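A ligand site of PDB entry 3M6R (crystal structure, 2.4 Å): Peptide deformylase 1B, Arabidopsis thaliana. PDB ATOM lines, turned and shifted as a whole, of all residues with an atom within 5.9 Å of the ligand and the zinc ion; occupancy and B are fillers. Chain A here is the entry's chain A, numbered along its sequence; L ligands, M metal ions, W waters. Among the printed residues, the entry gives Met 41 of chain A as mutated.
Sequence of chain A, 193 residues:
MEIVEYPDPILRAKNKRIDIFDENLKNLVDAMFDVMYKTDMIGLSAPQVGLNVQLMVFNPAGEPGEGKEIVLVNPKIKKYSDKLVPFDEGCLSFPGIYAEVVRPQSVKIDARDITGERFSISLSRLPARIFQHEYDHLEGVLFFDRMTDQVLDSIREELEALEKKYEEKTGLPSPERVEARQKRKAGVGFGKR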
ATOM      1  N   THR A  39      15.614 -18.639   7.252  1.00  0.00           N
ATOM      2  CA  THR A  39      14.822 -17.505   6.795  1.00  0.00           C
ATOM      3  C   THR A  39      13.569 -17.299   7.627  1.00  0.00           C
ATOM      4  O   THR A  39      12.737 -16.458   7.291  1.00  0.00           O
ATOM      5  CB  THR A  39      14.421 -17.656   5.302  1.00  0.00           C
ATOM      6  OG1 THR A  39      13.642 -18.842   5.127  1.00  0.00           O
ATOM      7  CG2 THR A  39      15.670 -17.742   4.419  1.00  0.00           C
ATOM      8  N   ASP A  40      13.448 -18.062   8.705  1.00  0.00           N
ATOM      9  CA  ASP A  40      12.287 -17.976   9.599  1.00  0.00           C
ATOM     10  C   ASP A  40      10.949 -18.268   8.930  1.00  0.00           C
ATOM     11  O   ASP A  40       9.945 -17.630   9.247  1.00  0.00           O
ATOM     12  CB  ASP A  40      12.229 -16.600  10.266  1.00  0.00           C
ATOM     13  CG  ASP A  40      12.811 -16.603  11.657  1.00  0.00           C
ATOM     14  OD1 ASP A  40      14.047 -16.771  11.796  1.00  0.00           O
ATOM     15  OD2 ASP A  40      12.030 -16.454  12.619  1.00  0.00           O
ATOM     16  N   MET A  41      10.924 -19.206   7.996  1.00  0.00           N
ATOM     17  CA  MET A  41       9.683 -19.560   7.325  1.00  0.00           C
ATOM     18  C   MET A  41       9.130 -20.844   7.964  1.00  0.00           C
ATOM     19  O   MET A  41       9.779 -21.445   8.808  1.00  0.00           O
ATOM     20  CB  MET A  41       9.926 -19.762   5.824  1.00  0.00           C
ATOM     21  CG  MET A  41      10.418 -18.513   5.071  1.00  0.00           C
ATOM     22  SD  MET A  41       9.444 -16.994   5.320  1.00  0.00           S
ATOM     23  CE  MET A  41       8.799 -16.727   3.853  1.00  0.00           C
ATOM     24  N   ILE A  42       7.920 -21.237   7.587  1.00  0.00           N
ATOM     25  CA  ILE A  42       7.362 -22.466   8.149  1.00  0.00           C
ATOM     26  C   ILE A  42       7.192 -23.511   7.071  1.00  0.00           C
ATOM     27  O   ILE A  42       6.702 -24.615   7.335  1.00  0.00           O
ATOM     28  CB  ILE A  42       6.009 -22.246   8.853  1.00  0.00           C
ATOM     29  CG1 ILE A  42       5.007 -21.594   7.905  1.00  0.00           C
ATOM     30  CG2 ILE A  42       6.214 -21.394  10.103  1.00  0.00           C
ATOM     31  CD1 ILE A  42       3.664 -21.319   8.537  1.00  0.00           C
ATOM     32  N   GLY A  43       7.611 -23.155   5.854  1.00  0.00           N
ATOM     33  CA  GLY A  43       7.515 -24.066   4.724  1.00  0.00           C
ATOM     34  C   GLY A  43       8.382 -23.603   3.567  1.00  0.00           C
ATOM     35  O   GLY A  43       8.881 -22.478   3.580  1.00  0.00           O
ATOM     36  N   LEU A  44       8.541 -24.453   2.565  1.00  0.00           N
ATOM     37  CA  LEU A  44       9.370 -24.104   1.415  1.00  0.00           C
ATOM     38  C   LEU A  44       9.137 -25.051   0.239  1.00  0.00           C
ATOM     39  O   LEU A  44       8.911 -26.253   0.430  1.00  0.00           O
ATOM     40  CB  LEU A  44      10.843 -24.121   1.831  1.00  0.00           C
ATOM     41  CG  LEU A  44      11.858 -23.456   0.914  1.00  0.00           C
ATOM     42  CD1 LEU A  44      11.506 -21.992   0.709  1.00  0.00           C
ATOM     43  CD2 LEU A  44      13.240 -23.601   1.538  1.00  0.00           C
ATOM     44  N   SER A  45       9.171 -24.519  -0.968  1.00  0.00           N
ATOM     45  CA  SER A  45       8.989 -25.351  -2.160  1.00  0.00           C
ATOM     46  C   SER A  45      10.269 -25.281  -2.992  1.00  0.00           C
ATOM     47  O   SER A  45      11.058 -24.353  -2.848  1.00  0.00           O
ATOM     48  CB  SER A  45       7.783 -24.895  -2.992  1.00  0.00           C
ATOM     49  OG  SER A  45       7.992 -23.605  -3.555  1.00  0.00           O
ATOM     50  N   GLN A  48      11.510 -22.130  -5.193  1.00  0.00           N
ATOM     51  CA  GLN A  48      12.038 -21.027  -4.420  1.00  0.00           C
ATOM     52  C   GLN A  48      13.537 -21.077  -4.180  1.00  0.00           C
ATOM     53  O   GLN A  48      14.151 -20.086  -3.756  1.00  0.00           O
ATOM     54  CB  GLN A  48      11.276 -20.935  -3.101  1.00  0.00           C
ATOM     55  CG  GLN A  48       9.821 -20.581  -3.302  1.00  0.00           C
ATOM     56  CD  GLN A  48       9.030 -20.583  -2.017  1.00  0.00           C
ATOM     57  OE1 GLN A  48       8.666 -21.638  -1.515  1.00  0.00           O
ATOM     58  NE2 GLN A  48       8.784 -19.390  -1.473  1.00  0.00           N
ATOM     59  N   PHE A  87      -7.000 -16.073   6.099  1.00  0.00           N
ATOM     60  CA  PHE A  87      -5.794 -16.168   6.914  1.00  0.00           C
ATOM     61  C   PHE A  87      -4.692 -15.321   6.270  1.00  0.00           C
ATOM     62  O   PHE A  87      -4.553 -15.288   5.049  1.00  0.00           O
ATOM     63  CB  PHE A  87      -5.385 -17.640   7.038  1.00  0.00           C
ATOM     64  CG  PHE A  87      -4.392 -17.900   8.127  1.00  0.00           C
ATOM     65  CD1 PHE A  87      -3.052 -18.105   7.826  1.00  0.00           C
ATOM     66  CD2 PHE A  87      -4.790 -17.924   9.457  1.00  0.00           C
ATOM     67  CE1 PHE A  87      -2.115 -18.326   8.850  1.00  0.00           C
ATOM     68  CE2 PHE A  87      -3.868 -18.140  10.484  1.00  0.00           C
ATOM     69  CZ  PHE A  87      -2.522 -18.336  10.169  1.00  0.00           C
ATOM     70  N   ASP A  88      -3.913 -14.610   7.079  1.00  0.00           N
ATOM     71  CA  ASP A  88      -2.850 -13.778   6.546  1.00  0.00           C
ATOM     72  C   ASP A  88      -1.641 -14.618   6.174  1.00  0.00           C
ATOM     73  O   ASP A  88      -1.245 -15.530   6.911  1.00  0.00           O
ATOM     74  CB  ASP A  88      -2.437 -12.688   7.542  1.00  0.00           C
ATOM     75  CG  ASP A  88      -3.500 -11.612   7.697  1.00  0.00           C
ATOM     76  OD1 ASP A  88      -4.053 -11.170   6.675  1.00  0.00           O
ATOM     77  OD2 ASP A  88      -3.759 -11.191   8.855  1.00  0.00           O
ATOM     78  N   GLU A  89      -1.050 -14.304   5.021  1.00  0.00           N
ATOM     79  CA  GLU A  89       0.089 -15.052   4.515  1.00  0.00           C
ATOM     80  C   GLU A  89       1.258 -14.193   4.081  1.00  0.00           C
ATOM     81  O   GLU A  89       1.089 -13.068   3.597  1.00  0.00           O
ATOM     82  CB  GLU A  89      -0.315 -15.907   3.320  1.00  0.00           C
ATOM     83  CG  GLU A  89      -1.099 -17.170   3.610  1.00  0.00           C
ATOM     84  CD  GLU A  89      -1.519 -17.888   2.339  1.00  0.00           C
ATOM     85  OE1 GLU A  89      -0.694 -17.962   1.391  1.00  0.00           O
ATOM     86  OE2 GLU A  89      -2.666 -18.380   2.262  1.00  0.00           O
ATOM     87  N   GLY A  90       2.453 -14.752   4.237  1.00  0.00           N
ATOM     88  CA  GLY A  90       3.662 -14.093   3.779  1.00  0.00           C
ATOM     89  C   GLY A  90       4.266 -15.064   2.762  1.00  0.00           C
ATOM     90  O   GLY A  90       3.734 -16.163   2.591  1.00  0.00           O
ATOM     91  N   CYS A  91       5.335 -14.684   2.070  1.00  0.00           N
ATOM     92  CA  CYS A  91       6.012 -15.569   1.110  1.00  0.00           C
ATOM     93  C   CYS A  91       7.473 -15.142   0.939  1.00  0.00           C
ATOM     94  O   CYS A  91       7.778 -13.960   0.669  1.00  0.00           O
ATOM     95  CB  CYS A  91       5.286 -15.559  -0.247  1.00  0.00           C
ATOM     96  SG  CYS A  91       5.949 -16.706  -1.555  1.00  0.00           S
ATOM     97  N   LEU A  92       8.377 -16.093   1.109  1.00  0.00           N
ATOM     98  CA  LEU A  92       9.807 -15.855   0.974  1.00  0.00           C
ATOM     99  C   LEU A  92      10.175 -15.283  -0.408  1.00  0.00           C
ATOM    100  O   LEU A  92      11.217 -14.654  -0.561  1.00  0.00           O
ATOM    101  CB  LEU A  92      10.567 -17.161   1.211  1.00  0.00           C
ATOM    102  CG  LEU A  92      12.094 -17.199   1.124  1.00  0.00           C
ATOM    103  CD1 LEU A  92      12.733 -16.388   2.266  1.00  0.00           C
ATOM    104  CD2 LEU A  92      12.537 -18.650   1.203  1.00  0.00           C
ATOM    105  N   SER A  93       9.331 -15.480  -1.409  1.00  0.00           N
ATOM    106  CA  SER A  93       9.639 -14.962  -2.728  1.00  0.00           C
ATOM    107  C   SER A  93       9.180 -13.507  -2.935  1.00  0.00           C
ATOM    108  O   SER A  93       9.502 -12.874  -3.939  1.00  0.00           O
ATOM    109  CB  SER A  93       9.060 -15.884  -3.803  1.00  0.00           C
ATOM    110  OG  SER A  93       9.587 -17.198  -3.689  1.00  0.00           O
ATOM    111  N   TYR A  98       2.583  -8.916   3.099  1.00  0.00           N
ATOM    112  CA  TYR A  98       1.644  -9.729   3.872  1.00  0.00           C
ATOM    113  C   TYR A  98       0.219  -9.365   3.488  1.00  0.00           C
ATOM    114  O   TYR A  98      -0.122  -8.194   3.354  1.00  0.00           O
ATOM    115  CB  TYR A  98       1.795  -9.498   5.369  1.00  0.00           C
ATOM    116  CG  TYR A  98       3.159  -9.800   5.888  1.00  0.00           C
ATOM    117  CD1 TYR A  98       3.393 -10.911   6.698  1.00  0.00           C
ATOM    118  CD2 TYR A  98       4.234  -8.950   5.588  1.00  0.00           C
ATOM    119  CE1 TYR A  98       4.680 -11.178   7.204  1.00  0.00           C
ATOM    120  CE2 TYR A  98       5.524  -9.204   6.089  1.00  0.00           C
ATOM    121  CZ  TYR A  98       5.731 -10.314   6.889  1.00  0.00           C
ATOM    122  OH  TYR A  98       7.006 -10.548   7.373  1.00  0.00           O
ATOM    123  N   ARG A 103      -8.697 -19.615   1.540  1.00  0.00           N
ATOM    124  CA  ARG A 103      -8.397 -20.945   1.015  1.00  0.00           C
ATOM    125  C   ARG A 103      -9.327 -21.934   1.691  1.00  0.00           C
ATOM    126  O   ARG A 103      -9.919 -21.621   2.715  1.00  0.00           O
ATOM    127  CB  ARG A 103      -6.940 -21.367   1.334  1.00  0.00           C
ATOM    128  CG  ARG A 103      -5.816 -20.599   0.609  1.00  0.00           C
ATOM    129  CD  ARG A 103      -4.443 -21.126   1.044  1.00  0.00           C
ATOM    130  NE  ARG A 103      -3.308 -20.307   0.593  1.00  0.00           N
ATOM    131  CZ  ARG A 103      -2.766 -20.339  -0.628  1.00  0.00           C
ATOM    132  NH1 ARG A 103      -1.732 -19.552  -0.911  1.00  0.00           N
ATOM    133  NH2 ARG A 103      -3.247 -21.143  -1.558  1.00  0.00           N
ATOM    134  N   LEU A 126      -3.758 -25.080  10.341  1.00  0.00           N
ATOM    135  CA  LEU A 126      -2.540 -24.534   9.789  1.00  0.00           C
ATOM    136  C   LEU A 126      -1.775 -25.435   8.799  1.00  0.00           C
ATOM    137  O   LEU A 126      -1.262 -24.970   7.777  1.00  0.00           O
ATOM    138  CB  LEU A 126      -1.617 -24.094  10.922  1.00  0.00           C
ATOM    139  CG  LEU A 126      -0.320 -23.403  10.493  1.00  0.00           C
ATOM    140  CD1 LEU A 126      -0.655 -22.126   9.725  1.00  0.00           C
ATOM    141  CD2 LEU A 126       0.522 -23.087  11.717  1.00  0.00           C
ATOM    142  N   ARG A 129      -3.071 -25.108   5.540  1.00  0.00           N
ATOM    143  CA  ARG A 129      -2.796 -23.789   5.023  1.00  0.00           C
ATOM    144  C   ARG A 129      -1.461 -23.723   4.321  1.00  0.00           C
ATOM    145  O   ARG A 129      -1.349 -23.178   3.221  1.00  0.00           O
ATOM    146  CB  ARG A 129      -2.749 -22.780   6.155  1.00  0.00           C
ATOM    147  CG  ARG A 129      -2.715 -21.393   5.617  1.00  0.00           C
ATOM    148  CD  ARG A 129      -4.024 -21.213   4.932  1.00  0.00           C
ATOM    149  NE  ARG A 129      -4.064 -19.993   4.165  1.00  0.00           N
ATOM    150  CZ  ARG A 129      -5.182 -19.337   3.907  1.00  0.00           C
ATOM    151  NH1 ARG A 129      -6.337 -19.802   4.371  1.00  0.00           N
ATOM    152  NH2 ARG A 129      -5.118 -18.220   3.210  1.00  0.00           N
ATOM    153  N   ILE A 130      -0.441 -24.250   4.998  1.00  0.00           N
ATOM    154  CA  ILE A 130       0.927 -24.293   4.519  1.00  0.00           C
ATOM    155  C   ILE A 130       1.022 -25.158   3.263  1.00  0.00           C
ATOM    156  O   ILE A 130       1.559 -24.741   2.251  1.00  0.00           O
ATOM    157  CB  ILE A 130       1.866 -24.878   5.610  1.00  0.00           C
ATOM    158  CG1 ILE A 130       1.740 -24.071   6.896  1.00  0.00           C
ATOM    159  CG2 ILE A 130       3.305 -24.883   5.128  1.00  0.00           C
ATOM    160  CD1 ILE A 130       2.548 -24.650   8.063  1.00  0.00           C
ATOM    161  N   HIS A 133      -0.329 -23.459   0.126  1.00  0.00           N
ATOM    162  CA  HIS A 133       0.508 -22.364  -0.330  1.00  0.00           C
ATOM    163  C   HIS A 133       1.673 -22.949  -1.159  1.00  0.00           C
ATOM    164  O   HIS A 133       2.022 -22.434  -2.223  1.00  0.00           O
ATOM    165  CB  HIS A 133       1.063 -21.608   0.878  1.00  0.00           C
ATOM    166  CG  HIS A 133       1.964 -20.466   0.530  1.00  0.00           C
ATOM    167  ND1 HIS A 133       1.482 -19.243   0.111  1.00  0.00           N
ATOM    168  CD2 HIS A 133       3.307 -20.361   0.535  1.00  0.00           C
ATOM    169  CE1 HIS A 133       2.499 -18.433  -0.107  1.00  0.00           C
ATOM    170  NE2 HIS A 133       3.615 -19.086   0.137  1.00  0.00           N
ATOM    171  N   GLU A 134       2.255 -24.038  -0.651  1.00  0.00           N
ATOM    172  CA  GLU A 134       3.375 -24.713  -1.309  1.00  0.00           C
ATOM    173  C   GLU A 134       2.902 -25.427  -2.579  1.00  0.00           C
ATOM    174  O   GLU A 134       3.519 -25.329  -3.636  1.00  0.00           O
ATOM    175  CB  GLU A 134       3.997 -25.723  -0.351  1.00  0.00           C
ATOM    176  CG  GLU A 134       4.276 -25.181   1.038  1.00  0.00           C
ATOM    177  CD  GLU A 134       5.302 -24.054   1.054  1.00  0.00           C
ATOM    178  OE1 GLU A 134       5.360 -23.324   2.071  1.00  0.00           O
ATOM    179  OE2 GLU A 134       6.058 -23.907   0.074  1.00  0.00           O
ATOM    180  N   HIS A 137       2.691 -23.260  -5.236  1.00  0.00           N
ATOM    181  CA  HIS A 137       4.037 -23.044  -5.725  1.00  0.00           C
ATOM    182  C   HIS A 137       4.460 -24.107  -6.741  1.00  0.00           C
ATOM    183  O   HIS A 137       4.991 -23.781  -7.804  1.00  0.00           O
ATOM    184  CB  HIS A 137       5.038 -23.052  -4.571  1.00  0.00           C
ATOM    185  CG  HIS A 137       5.391 -21.703  -4.051  1.00  0.00           C
ATOM    186  ND1 HIS A 137       6.049 -20.753  -4.813  1.00  0.00           N
ATOM    187  CD2 HIS A 137       5.216 -21.146  -2.823  1.00  0.00           C
ATOM    188  CE1 HIS A 137       6.270 -19.675  -4.076  1.00  0.00           C
ATOM    189  NE2 HIS A 137       5.773 -19.898  -2.861  1.00  0.00           N
HETATM  190  C1  LIG L   1       7.116 -19.496   3.241  1.00  0.00           C
HETATM  191  C2  LIG L   1       6.854 -20.092   1.767  1.00  0.00           C
HETATM  192  O1  LIG L   1       7.056 -19.057   1.117  1.00  0.00           O
HETATM  193  N1  LIG L   1       6.562 -21.241   1.158  1.00  0.00           N
HETATM  194  O2  LIG L   1       6.425 -21.293  -0.223  1.00  0.00           O
HETATM  195  C3  LIG L   1       5.684 -19.041   3.699  1.00  0.00           C
HETATM  196  C4  LIG L   1       5.973 -18.496   5.137  1.00  0.00           C
HETATM  197  O3  LIG L   1       6.617 -19.206   5.927  1.00  0.00           O
HETATM  198  C5  LIG L   1       4.738 -20.273   3.791  1.00  0.00           C
HETATM  199  C6  LIG L   1       3.340 -19.746   4.214  1.00  0.00           C
HETATM  200  C7  LIG L   1       2.313 -20.822   4.374  1.00  0.00           C
HETATM  201  C8  LIG L   1       0.976 -20.127   4.557  1.00  0.00           C
HETATM  202  C9  LIG L   1       0.754 -19.772   6.023  1.00  0.00           C
HETATM  203  N2  LIG L   1       5.428 -17.241   5.320  1.00  0.00           N
HETATM  204  C10 LIG L   1       5.009 -17.154   6.751  1.00  0.00           C
HETATM  205  C11 LIG L   1       5.793 -15.875   7.296  1.00  0.00           C
HETATM  206  C12 LIG L   1       7.257 -16.207   7.702  1.00  0.00           C
HETATM  207  C13 LIG L   1       5.828 -14.703   6.250  1.00  0.00           C
HETATM  208  C14 LIG L   1       3.474 -16.908   6.955  1.00  0.00           C
HETATM  209  O4  LIG L   1       2.761 -16.751   5.992  1.00  0.00           O
HETATM  210  N3  LIG L   1       3.231 -17.018   8.496  1.00  0.00           N
HETATM  211  C15 LIG L   1       1.840 -16.862   9.027  1.00  0.00           C
HETATM  212  C16 LIG L   1       4.118 -17.289   9.691  1.00  0.00           C
HETATM  213  C17 LIG L   1       3.169 -17.958  10.708  1.00  0.00           C
HETATM  214  C18 LIG L   1       1.933 -17.049  10.560  1.00  0.00           C
HETATM  215  C19 LIG L   1       1.288 -15.450   8.723  1.00  0.00           C
HETATM  216  O5  LIG L   1      -0.042 -15.309   9.214  1.00  0.00           O
HETATM  217 ZN    ZN M   1       5.605 -18.970  -0.810  1.00  0.00          ZN
HETATM  218  O   HOH W   1       0.733 -11.961   9.700  1.00  0.00           O
HETATM  219  O   HOH W   2       2.071 -16.752  13.764  1.00  0.00           O
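Residues that only touch the zinc ion: Gln 48 (3.3 Å). Four residues have an atom within 4 Å of the zinc ion: Gln 48, Cys 91, His 133 and His 137. The nearest printed residue that does not touch the zinc ion is Leu 92 (4.4 Å).
The zinc ion is bound by a ring nitrogen (NE2) of His 133 (2.2 Å), a ring nitrogen (NE2) of His 137 (2.3 Å), the side-chain sulfur (SG) of Cys 91 (2.4 Å), an oxygen (O1) of the ligand (2.4 Å) and an oxygen (O2) of the ligand (2.5 Å). The zinc ion has five donor atoms within binding distance.
A ring nitrogen (ND1) of His 133 is in hydrogen-bond range of the side-chain carboxylate (OE1) of Glu 89, at 2.8 Å. The side-chain amide nitrogen (NE2) of Gln 48 sits close to a ring nitrogen (NE2) of His 137. The backbone NH (N) of Ser 93 lies close to the side-chain sulfur (SG) of Cys 91, 3.6 Å away. The backbone NH (N) of Leu 44 is in hydrogen-bond range of the side-chain carboxylate (OE1) of Glu 134 (3.4 Å). OE1 of Gln 48 is in hydrogen-bond range of OG of Ser 45 (2.9 Å). NE2 of Gln 48 sits at hydrogen-bond distance from OG of Ser 93, at 3.2 Å. OE2 of Glu 89 lies within salt-bridge range of NH2 of Arg 129, 2.6 Å away. The guanidinium group (NE) of Arg 103 is in salt-bridge range of the side-chain carboxylate (OE2) of Glu 89, 2.6 Å away.
The side-chain carboxylate (OE1) of Glu 134 is in hydrogen-bond range of a nitrogen (N1) of the ligand (2.6 Å). O5 of the ligand is in hydrogen-bond range of O of Asp 88 (2.6 Å). The side-chain amide oxygen (OE1) of Gln 48 lies within hydrogen-bond range of a nitrogen (N1) of the ligand, 3.4 Å away. N of Gly 90 is in hydrogen-bond range of O4 of the ligand, at 2.7 Å. O of Gly 90 is in hydrogen-bond range of N2 of the ligand, at 3.4 Å. The backbone NH of Ile 42 sits at hydrogen-bond distance from an oxygen (O3) of the ligand, 2.9 Å away. The backbone NH (N) of Leu 92 lies close to an oxygen (O1) of the ligand (3.2 Å).
The side-chain sulfur (SD) of Met 41 sits close to an oxygen (O3) of the ligand, at 3.6 Å. O of Asp 40 touches C12 of the ligand, at 3.4 Å. O of Gly 43 touches C1 of the ligand (3.5 Å). Phe 87 touches the ligand (CE1 to O5, 3.7 Å). Glu 89 touches the ligand (CA to O4, 3.5 Å). Tyr 98 touches the ligand. Arg 129 touches the ligand (CG to C9, 3.9 Å). Ile 130 touches the ligand (CA to C7, 3.7 Å). Hydrophobic or aromatic side chains that line the ligand: Met 41, Ile 42, Phe 87, Leu 92, Tyr 98, His 133 and His 137. Within 4 Å of the ligand: Asp 40, Met 41, Ile 42, Gly 43, Gln 48, Phe 87, Asp 88, Glu 89, Gly 90, Cys 91, Leu 92, Tyr 98, Arg 129, Ile 130, His 133, Glu 134 and His 137. The nearest printed residue that does not touch the ligand is Leu 44 (4.02 Å).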
